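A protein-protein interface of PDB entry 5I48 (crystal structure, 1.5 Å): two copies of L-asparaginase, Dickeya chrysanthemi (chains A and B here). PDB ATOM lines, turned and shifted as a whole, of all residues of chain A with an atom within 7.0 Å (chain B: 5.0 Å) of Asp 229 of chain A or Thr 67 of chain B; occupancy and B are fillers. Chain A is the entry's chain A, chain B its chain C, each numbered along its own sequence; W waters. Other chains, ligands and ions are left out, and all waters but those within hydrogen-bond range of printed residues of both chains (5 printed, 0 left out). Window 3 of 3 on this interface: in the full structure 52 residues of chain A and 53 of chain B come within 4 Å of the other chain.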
ATOM      1  N   TYR A 227       4.070  20.885  15.963  1.00  0.00           N
ATOM      2  CA  TYR A 227       3.299  20.511  14.779  1.00  0.00           C
ATOM      3  C   TYR A 227       1.861  20.887  15.013  1.00  0.00           C
ATOM      4  O   TYR A 227       1.454  21.172  16.156  1.00  0.00           O
ATOM      5  CB  TYR A 227       3.420  19.048  14.454  1.00  0.00           C
ATOM      6  CG  TYR A 227       3.128  18.096  15.628  1.00  0.00           C
ATOM      7  CD1 TYR A 227       4.078  17.893  16.632  1.00  0.00           C
ATOM      8  CD2 TYR A 227       1.942  17.429  15.730  1.00  0.00           C
ATOM      9  CE1 TYR A 227       3.855  17.024  17.696  1.00  0.00           C
ATOM     10  CE2 TYR A 227       1.711  16.547  16.767  1.00  0.00           C
ATOM     11  CZ  TYR A 227       2.655  16.350  17.754  1.00  0.00           C
ATOM     12  OH  TYR A 227       2.469  15.454  18.800  1.00  0.00           O
ATOM     13  N   GLN A 228       1.077  20.814  13.935  1.00  0.00           N
ATOM     14  CA  GLN A 228      -0.357  21.089  14.081  1.00  0.00           C
ATOM     15  C   GLN A 228      -0.951  20.112  15.089  1.00  0.00           C
ATOM     16  O   GLN A 228      -0.664  18.937  15.045  1.00  0.00           O
ATOM     17  CB  GLN A 228      -1.072  20.923  12.785  1.00  0.00           C
ATOM     18  CG  GLN A 228      -0.797  22.018  11.755  1.00  0.00           C
ATOM     19  CD  GLN A 228      -1.630  21.897  10.477  1.00  0.00           C
ATOM     20  OE1 GLN A 228      -2.339  20.903  10.266  1.00  0.00           O
ATOM     21  NE2 GLN A 228      -1.510  22.901   9.591  1.00  0.00           N
ATOM     22  N   ASP A 229      -1.782  20.652  15.995  1.00  0.00           N
ATOM     23  CA  ASP A 229      -2.437  19.812  17.082  1.00  0.00           C
ATOM     24  C   ASP A 229      -1.469  19.208  18.089  1.00  0.00           C
ATOM     25  O   ASP A 229      -1.811  18.246  18.804  1.00  0.00           O
ATOM     26  CB  ASP A 229      -3.192  18.655  16.484  1.00  0.00           C
ATOM     27  CG  ASP A 229      -4.304  19.115  15.517  1.00  0.00           C
ATOM     28  OD1 ASP A 229      -5.212  19.882  15.944  1.00  0.00           O
ATOM     29  OD2 ASP A 229      -4.200  18.774  14.280  1.00  0.00           O
ATOM     30  N   ASP A 230      -0.299  19.796  18.218  1.00  0.00           N
ATOM     31  CA  ASP A 230       0.630  19.313  19.208  1.00  0.00           C
ATOM     32  C   ASP A 230       0.003  19.327  20.628  1.00  0.00           C
ATOM     33  O   ASP A 230      -0.655  20.312  21.020  1.00  0.00           O
ATOM     34  CB  ASP A 230       1.955  20.085  19.208  1.00  0.00           C
ATOM     35  CG  ASP A 230       1.838  21.554  19.516  1.00  0.00           C
ATOM     36  OD1 ASP A 230       0.785  22.242  19.273  1.00  0.00           O
ATOM     37  OD2 ASP A 230       2.860  22.071  19.988  1.00  0.00           O
ATOM     38  N   PRO A 231       0.254  18.278  21.426  1.00  0.00           N
ATOM     39  CA  PRO A 231      -0.476  18.210  22.686  1.00  0.00           C
ATOM     40  C   PRO A 231       0.221  18.760  23.871  1.00  0.00           C
ATOM     41  O   PRO A 231       1.404  18.601  24.068  1.00  0.00           O
ATOM     42  CB  PRO A 231      -0.630  16.733  22.879  1.00  0.00           C
ATOM     43  CG  PRO A 231       0.648  16.141  22.240  1.00  0.00           C
ATOM     44  CD  PRO A 231       0.872  16.996  21.051  1.00  0.00           C
ATOM     45  N   GLU A 232      -0.597  19.322  24.760  1.00  0.00           N
ATOM     46  CA  GLU A 232      -0.098  19.827  26.029  1.00  0.00           C
ATOM     47  C   GLU A 232       0.365  18.661  26.908  1.00  0.00           C
ATOM     48  O   GLU A 232       1.329  18.899  27.686  1.00  0.00           O
ATOM     49  CB  GLU A 232      -1.222  20.696  26.667  1.00  0.00           C
ATOM     50  CG  GLU A 232      -0.791  21.459  27.866  1.00  0.00           C
ATOM     51  CD  GLU A 232      -1.909  22.307  28.441  1.00  0.00           C
ATOM     52  OE1 GLU A 232      -2.932  22.621  27.772  1.00  0.00           O
ATOM     53  OE2 GLU A 232      -1.697  22.691  29.580  1.00  0.00           O
ATOM     54  N   MET A 251       7.776  24.795  15.295  1.00  0.00           N
ATOM     55  CA  MET A 251       7.310  25.139  13.993  1.00  0.00           C
ATOM     56  C   MET A 251       8.009  26.429  13.583  1.00  0.00           C
ATOM     57  O   MET A 251       8.090  27.342  14.342  1.00  0.00           O
ATOM     58  CB  MET A 251       5.764  25.326  14.003  1.00  0.00           C
ATOM     59  CG  MET A 251       5.053  24.007  14.335  1.00  0.00           C
ATOM     60  SD  MET A 251       3.302  24.195  14.698  1.00  0.00           S
ATOM     61  CE  MET A 251       3.343  24.538  16.464  1.00  0.00           C
ATOM     62  N   SER A 257       2.164  26.874  19.504  1.00  0.00           N
ATOM     63  CA  SER A 257       0.652  26.883  19.540  1.00  0.00           C
ATOM     64  C   SER A 257       0.162  27.290  20.863  1.00  0.00           C
ATOM     65  O   SER A 257       0.931  27.318  21.865  1.00  0.00           O
ATOM     66  CB  SER A 257       0.114  25.518  19.206  1.00  0.00           C
ATOM     67  OG  SER A 257       0.310  24.634  20.308  1.00  0.00           O
ATOM     68  N   ARG A 259      -1.445  25.476  22.834  1.00  0.00           N
ATOM     69  CA  ARG A 259      -1.188  24.295  23.689  1.00  0.00           C
ATOM     70  C   ARG A 259       0.241  24.212  24.132  1.00  0.00           C
ATOM     71  O   ARG A 259       0.547  23.963  25.295  1.00  0.00           O
ATOM     72  CB  ARG A 259      -1.616  23.062  22.952  1.00  0.00           C
ATOM     73  CG  ARG A 259      -3.101  23.011  22.576  1.00  0.00           C
ATOM     74  CD  ARG A 259      -3.471  21.828  21.702  1.00  0.00           C
ATOM     75  NE  ARG A 259      -2.726  21.929  20.472  1.00  0.00           N
ATOM     76  CZ  ARG A 259      -2.859  22.808  19.511  1.00  0.00           C
ATOM     77  NH1 ARG A 259      -3.911  23.557  19.391  1.00  0.00           N
ATOM     78  NH2 ARG A 259      -1.987  22.847  18.546  1.00  0.00           N
ATOM     79  N   ASN B  65      -1.123  27.765  14.978  1.00  0.00           N
ATOM     80  CA  ASN B  65      -2.407  27.442  15.609  1.00  0.00           C
ATOM     81  C   ASN B  65      -3.394  26.730  14.738  1.00  0.00           C
ATOM     82  O   ASN B  65      -4.489  26.353  15.189  1.00  0.00           O
ATOM     83  CB  ASN B  65      -3.015  28.716  16.262  1.00  0.00           C
ATOM     84  CG  ASN B  65      -2.285  28.995  17.552  1.00  0.00           C
ATOM     85  OD1 ASN B  65      -2.199  28.083  18.427  1.00  0.00           O
ATOM     86  ND2 ASN B  65      -1.806  30.156  17.713  1.00  0.00           N
ATOM     87  N   MET B  66      -3.007  26.458  13.523  1.00  0.00           N
ATOM     88  CA  MET B  66      -3.846  25.676  12.609  1.00  0.00           C
ATOM     89  C   MET B  66      -3.966  24.228  13.140  1.00  0.00           C
ATOM     90  O   MET B  66      -3.020  23.630  13.564  1.00  0.00           O
ATOM     91  CB  MET B  66      -3.262  25.726  11.234  1.00  0.00           C
ATOM     92  CG  MET B  66      -4.079  25.023  10.166  1.00  0.00           C
ATOM     93  SD  MET B  66      -5.717  25.719   9.904  1.00  0.00           S
ATOM     94  CE  MET B  66      -5.430  27.404   9.372  1.00  0.00           C
ATOM     95  N   THR B  67      -5.185  23.704  13.113  1.00  0.00           N
ATOM     96  CA  THR B  67      -5.515  22.396  13.595  1.00  0.00           C
ATOM     97  C   THR B  67      -6.142  21.583  12.535  1.00  0.00           C
ATOM     98  O   THR B  67      -6.728  22.091  11.612  1.00  0.00           O
ATOM     99  CB  THR B  67      -6.452  22.473  14.755  1.00  0.00           C
ATOM    100  OG1 THR B  67      -7.627  23.263  14.392  1.00  0.00           O
ATOM    101  CG2 THR B  67      -5.792  23.121  15.931  1.00  0.00           C
ATOM    102  N   GLY B  68      -6.012  20.257  12.640  1.00  0.00           N
ATOM    103  CA  GLY B  68      -6.570  19.343  11.674  1.00  0.00           C
ATOM    104  C   GLY B  68      -8.055  19.556  11.474  1.00  0.00           C
ATOM    105  O   GLY B  68      -8.524  19.456  10.365  1.00  0.00           O
ATOM    106  N   ASP B  69      -8.803  19.822  12.527  1.00  0.00           N
ATOM    107  CA  ASP B  69     -10.306  20.054  12.302  1.00  0.00           C
ATOM    108  C   ASP B  69     -10.580  21.211  11.408  1.00  0.00           C
ATOM    109  O   ASP B  69     -11.486  21.176  10.597  1.00  0.00           O
ATOM    110  CB  ASP B  69     -11.017  20.261  13.652  1.00  0.00           C
ATOM    111  CG  ASP B  69     -11.034  18.952  14.541  1.00  0.00           C
ATOM    112  OD1 ASP B  69     -10.827  17.791  14.027  1.00  0.00           O
ATOM    113  OD2 ASP B  69     -11.215  19.099  15.772  1.00  0.00           O
ATOM    114  N   VAL B  70      -9.736  22.227  11.502  1.00  0.00           N
ATOM    115  CA  VAL B  70      -9.869  23.389  10.625  1.00  0.00           C
ATOM    116  C   VAL B  70      -9.363  23.107   9.219  1.00  0.00           C
ATOM    117  O   VAL B  70      -9.976  23.513   8.252  1.00  0.00           O
ATOM    118  CB  VAL B  70      -9.199  24.634  11.244  1.00  0.00           C
ATOM    119  CG1 VAL B  70      -9.196  25.782  10.298  1.00  0.00           C
ATOM    120  CG2 VAL B  70      -9.915  25.008  12.561  1.00  0.00           C
ATOM    121  N   VAL B  71      -8.235  22.345   9.078  1.00  0.00           N
ATOM    122  CA  VAL B  71      -7.764  21.952   7.803  1.00  0.00           C
ATOM    123  C   VAL B  71      -8.794  21.118   7.044  1.00  0.00           C
ATOM    124  O   VAL B  71      -8.945  21.197   5.853  1.00  0.00           O
ATOM    125  CB  VAL B  71      -6.421  21.192   7.885  1.00  0.00           C
ATOM    126  CG1 VAL B  71      -5.941  20.809   6.511  1.00  0.00           C
ATOM    127  CG2 VAL B  71      -5.367  22.080   8.578  1.00  0.00           C
ATOM    128  N   LYS B 220      -6.116  10.786  16.163  1.00  0.00           N
ATOM    129  CA  LYS B 220      -5.094  11.496  16.955  1.00  0.00           C
ATOM    130  C   LYS B 220      -3.729  10.855  16.599  1.00  0.00           C
ATOM    131  O   LYS B 220      -3.535   9.614  16.725  1.00  0.00           O
ATOM    132  CB  LYS B 220      -5.398  11.340  18.376  1.00  0.00           C
ATOM    133  CG  LYS B 220      -4.450  12.093  19.243  1.00  0.00           C
ATOM    134  CD  LYS B 220      -4.889  12.206  20.691  1.00  0.00           C
ATOM    135  CE  LYS B 220      -3.757  12.917  21.483  1.00  0.00           C
ATOM    136  NZ  LYS B 220      -3.126  14.219  20.978  1.00  0.00           N
ATOM    137  N   ASP B 222       0.475  11.632  17.193  1.00  0.00           N
ATOM    138  CA  ASP B 222       1.543  12.487  17.767  1.00  0.00           C
ATOM    139  C   ASP B 222       2.902  12.202  17.135  1.00  0.00           C
ATOM    140  O   ASP B 222       3.060  11.167  16.533  1.00  0.00           O
ATOM    141  CB  ASP B 222       1.564  12.372  19.308  1.00  0.00           C
ATOM    142  CG  ASP B 222       0.391  13.189  19.926  1.00  0.00           C
ATOM    143  OD1 ASP B 222       0.000  14.237  19.344  1.00  0.00           O
ATOM    144  OD2 ASP B 222      -0.133  12.763  20.920  1.00  0.00           O
ATOM    145  N   ARG B 305       2.764  12.539   9.469  1.00  0.00           N
ATOM    146  CA  ARG B 305       1.624  12.570  10.392  1.00  0.00           C
ATOM    147  C   ARG B 305       0.345  12.792   9.609  1.00  0.00           C
ATOM    148  O   ARG B 305      -0.685  12.156   9.882  1.00  0.00           O
ATOM    149  CB  ARG B 305       1.825  13.672  11.477  1.00  0.00           C
ATOM    150  CG  ARG B 305       0.583  14.075  12.205  1.00  0.00           C
ATOM    151  CD  ARG B 305       0.839  15.012  13.383  1.00  0.00           C
ATOM    152  NE  ARG B 305      -0.454  15.329  13.976  1.00  0.00           N
ATOM    153  CZ  ARG B 305      -1.313  16.189  13.488  1.00  0.00           C
ATOM    154  NH1 ARG B 305      -0.964  16.941  12.476  1.00  0.00           N
ATOM    155  NH2 ARG B 305      -2.493  16.331  14.060  1.00  0.00           N
ATOM    156  N   MET B 309      -2.683  10.162   9.591  1.00  0.00           N
ATOM    157  CA  MET B 309      -3.988  10.546  10.035  1.00  0.00           C
ATOM    158  C   MET B 309      -5.052  10.180   8.980  1.00  0.00           C
ATOM    159  O   MET B 309      -6.088   9.590   9.326  1.00  0.00           O
ATOM    160  CB  MET B 309      -4.132  12.006  10.278  1.00  0.00           C
ATOM    161  CG  MET B 309      -3.407  12.442  11.420  1.00  0.00           C
ATOM    162  SD  MET B 309      -3.343  14.266  11.452  1.00  0.00           S
ATOM    163  CE  MET B 309      -4.888  14.404  12.008  1.00  0.00           C
HETATM  164  O   HOH W   1      -7.762  19.100  15.179  1.00  0.00           O
HETATM  165  O   HOH W   2      -4.400  25.978  17.874  1.00  0.00           O
HETATM  166  O   HOH W   3      -2.167  15.430  18.515  1.00  0.00           O
HETATM  167  O   HOH W   4      -1.795  23.950  15.935  1.00  0.00           O
HETATM  168  O   HOH W   5      -3.205  18.596  11.525  1.00  0.00           O
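Of the 11 printed residues of chain B, 7 touch a printed residue of chain A. Among the printed residues, Asp or Glu carboxylates within 4 Å of a Lys or Arg side-chain nitrogen of the other chain: Asp 229 of chain A with Arg 305 of chain B (3.0 Å).
Water W3 lies within hydrogen-bond range of OD1 of Asp 222 of chain B (2.6 Å), O of Asp 229 of chain A (2.9 Å) and NZ of Lys 220 of chain B (2.9 Å). Water W4 lies within hydrogen-bond range of the backbone carbonyl oxygen (O) of Met 66 of chain B (2.7 Å), the guanidinium group (NH2) of Arg 259 of chain A (2.8 Å) and the backbone NH (N) of Asp 229 of chain A (3.3 Å). Water W2 bridges O of Asn 65 of chain B (2.7 Å) and NH1 of Arg 259 of chain A (2.9 Å). Water W5 lies within hydrogen-bond range of OE1 of Gln 228 of chain A (2.8 Å), OD2 of Asp 229 of chain A (2.9 Å), NH1 of Arg 305 of chain B (2.9 Å) and N of Gly 68 of chain B (3.4 Å). Water W1 lies within hydrogen-bond range of the side-chain carboxylate of Asp 229 of chain A (2.8 Å), the backbone NH of Asp 69 of chain B (2.9 Å) and the backbone NH of Gly 68 of chain B (3.3 Å).
The guanidinium group of Arg 305 of chain B lies within salt-bridge range of the side-chain carboxylate of Asp 229 of chain A (3.0 Å). The side-chain hydroxyl (OH) of Tyr 227 of chain A lies within hydrogen-bond range of the side-chain carboxylate (OD1) of Asp 222 of chain B (2.8 Å). OD2 of Asp 229 of chain A is in hydrogen-bond range of N of Gly 68 of chain B (2.9 Å). O of Gln 228 of chain A sits close to NH1 of Arg 305 of chain B, 3.3 Å away.
Among the printed residues, pairs that only touch across the chains: Tyr 227 of chain A with Arg 305 of chain B, Gln 228 of chain A with Met 66 of chain B, Gln 228 of chain A with Val 71 of chain B, Asp 229 of chain A with Thr 67 of chain B, Pro 231 of chain A with Asp 222 of chain B, Ser 257 of chain A with Asn 65 of chain B and Arg 259 of chain A with Thr 67 of chain B.
The side-chain carboxylate (OD1) of Asp 230 of chain A lies within hydrogen-bond range of the side-chain hydroxyl (OG) of Ser 257 of chain A (2.6 Å). OG of Ser 257 of chain A lies close to N of Arg 259 of chain A, at 3.2 Å. N of Tyr 227 of chain A lies close to SD of Met 251 of chain A (3.6 Å). OD1 of Asp 230 of chain A is in salt-bridge range of NH2 of Arg 259 of chain A (2.9 Å). NZ of Lys 220 of chain B is in salt-bridge range of OD2 of Asp 222 of chain B (3.3 Å). The guanidinium group (NH2) of Arg 305 of chain B sits at hydrogen-bond distance from the side-chain sulfur (SD) of Met 309 of chain B, at 3.4 Å.
No position is printed for both chains. Of the 11 pairs that touch across the chains among the printed residues, none has its exchanged pair printed and touching as well.
Printed residues of chain B within 4 Å of Gln 228 of chain A: Met 66 (3.3 Å), Val 71 (3.7 Å) and Arg 305 (3.2 Å). Of chain B, only Thr 67 (3.1 Å), Gly 68 (2.9 Å) and Arg 305 (3.0 Å) come within 4 Å of Asp 229 of chain A. Of the printed residues of chain A, Met 66 of chain B touches Gln 228 (3.3 Å). Of the printed residues of chain A, Thr 67 of chain B touches Asp 229 (3.1 Å) and Arg 259 (3.96 Å). Of the printed residues of chain A, Val 71 of chain B touches Gln 228. Lys 220 of chain B touches none of the printed residues of chain A. Of the printed residues of chain A, Asp 222 of chain B touches Tyr 227 (2.8 Å) and Pro 231 (3.4 Å). Of the printed residues of chain A, Arg 305 of chain B touches Tyr 227, Gln 228 and Asp 229. The nearest printed residue of chain B that does not touch Tyr 227 of chain A is Met 66 of chain B (5.7 Å).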
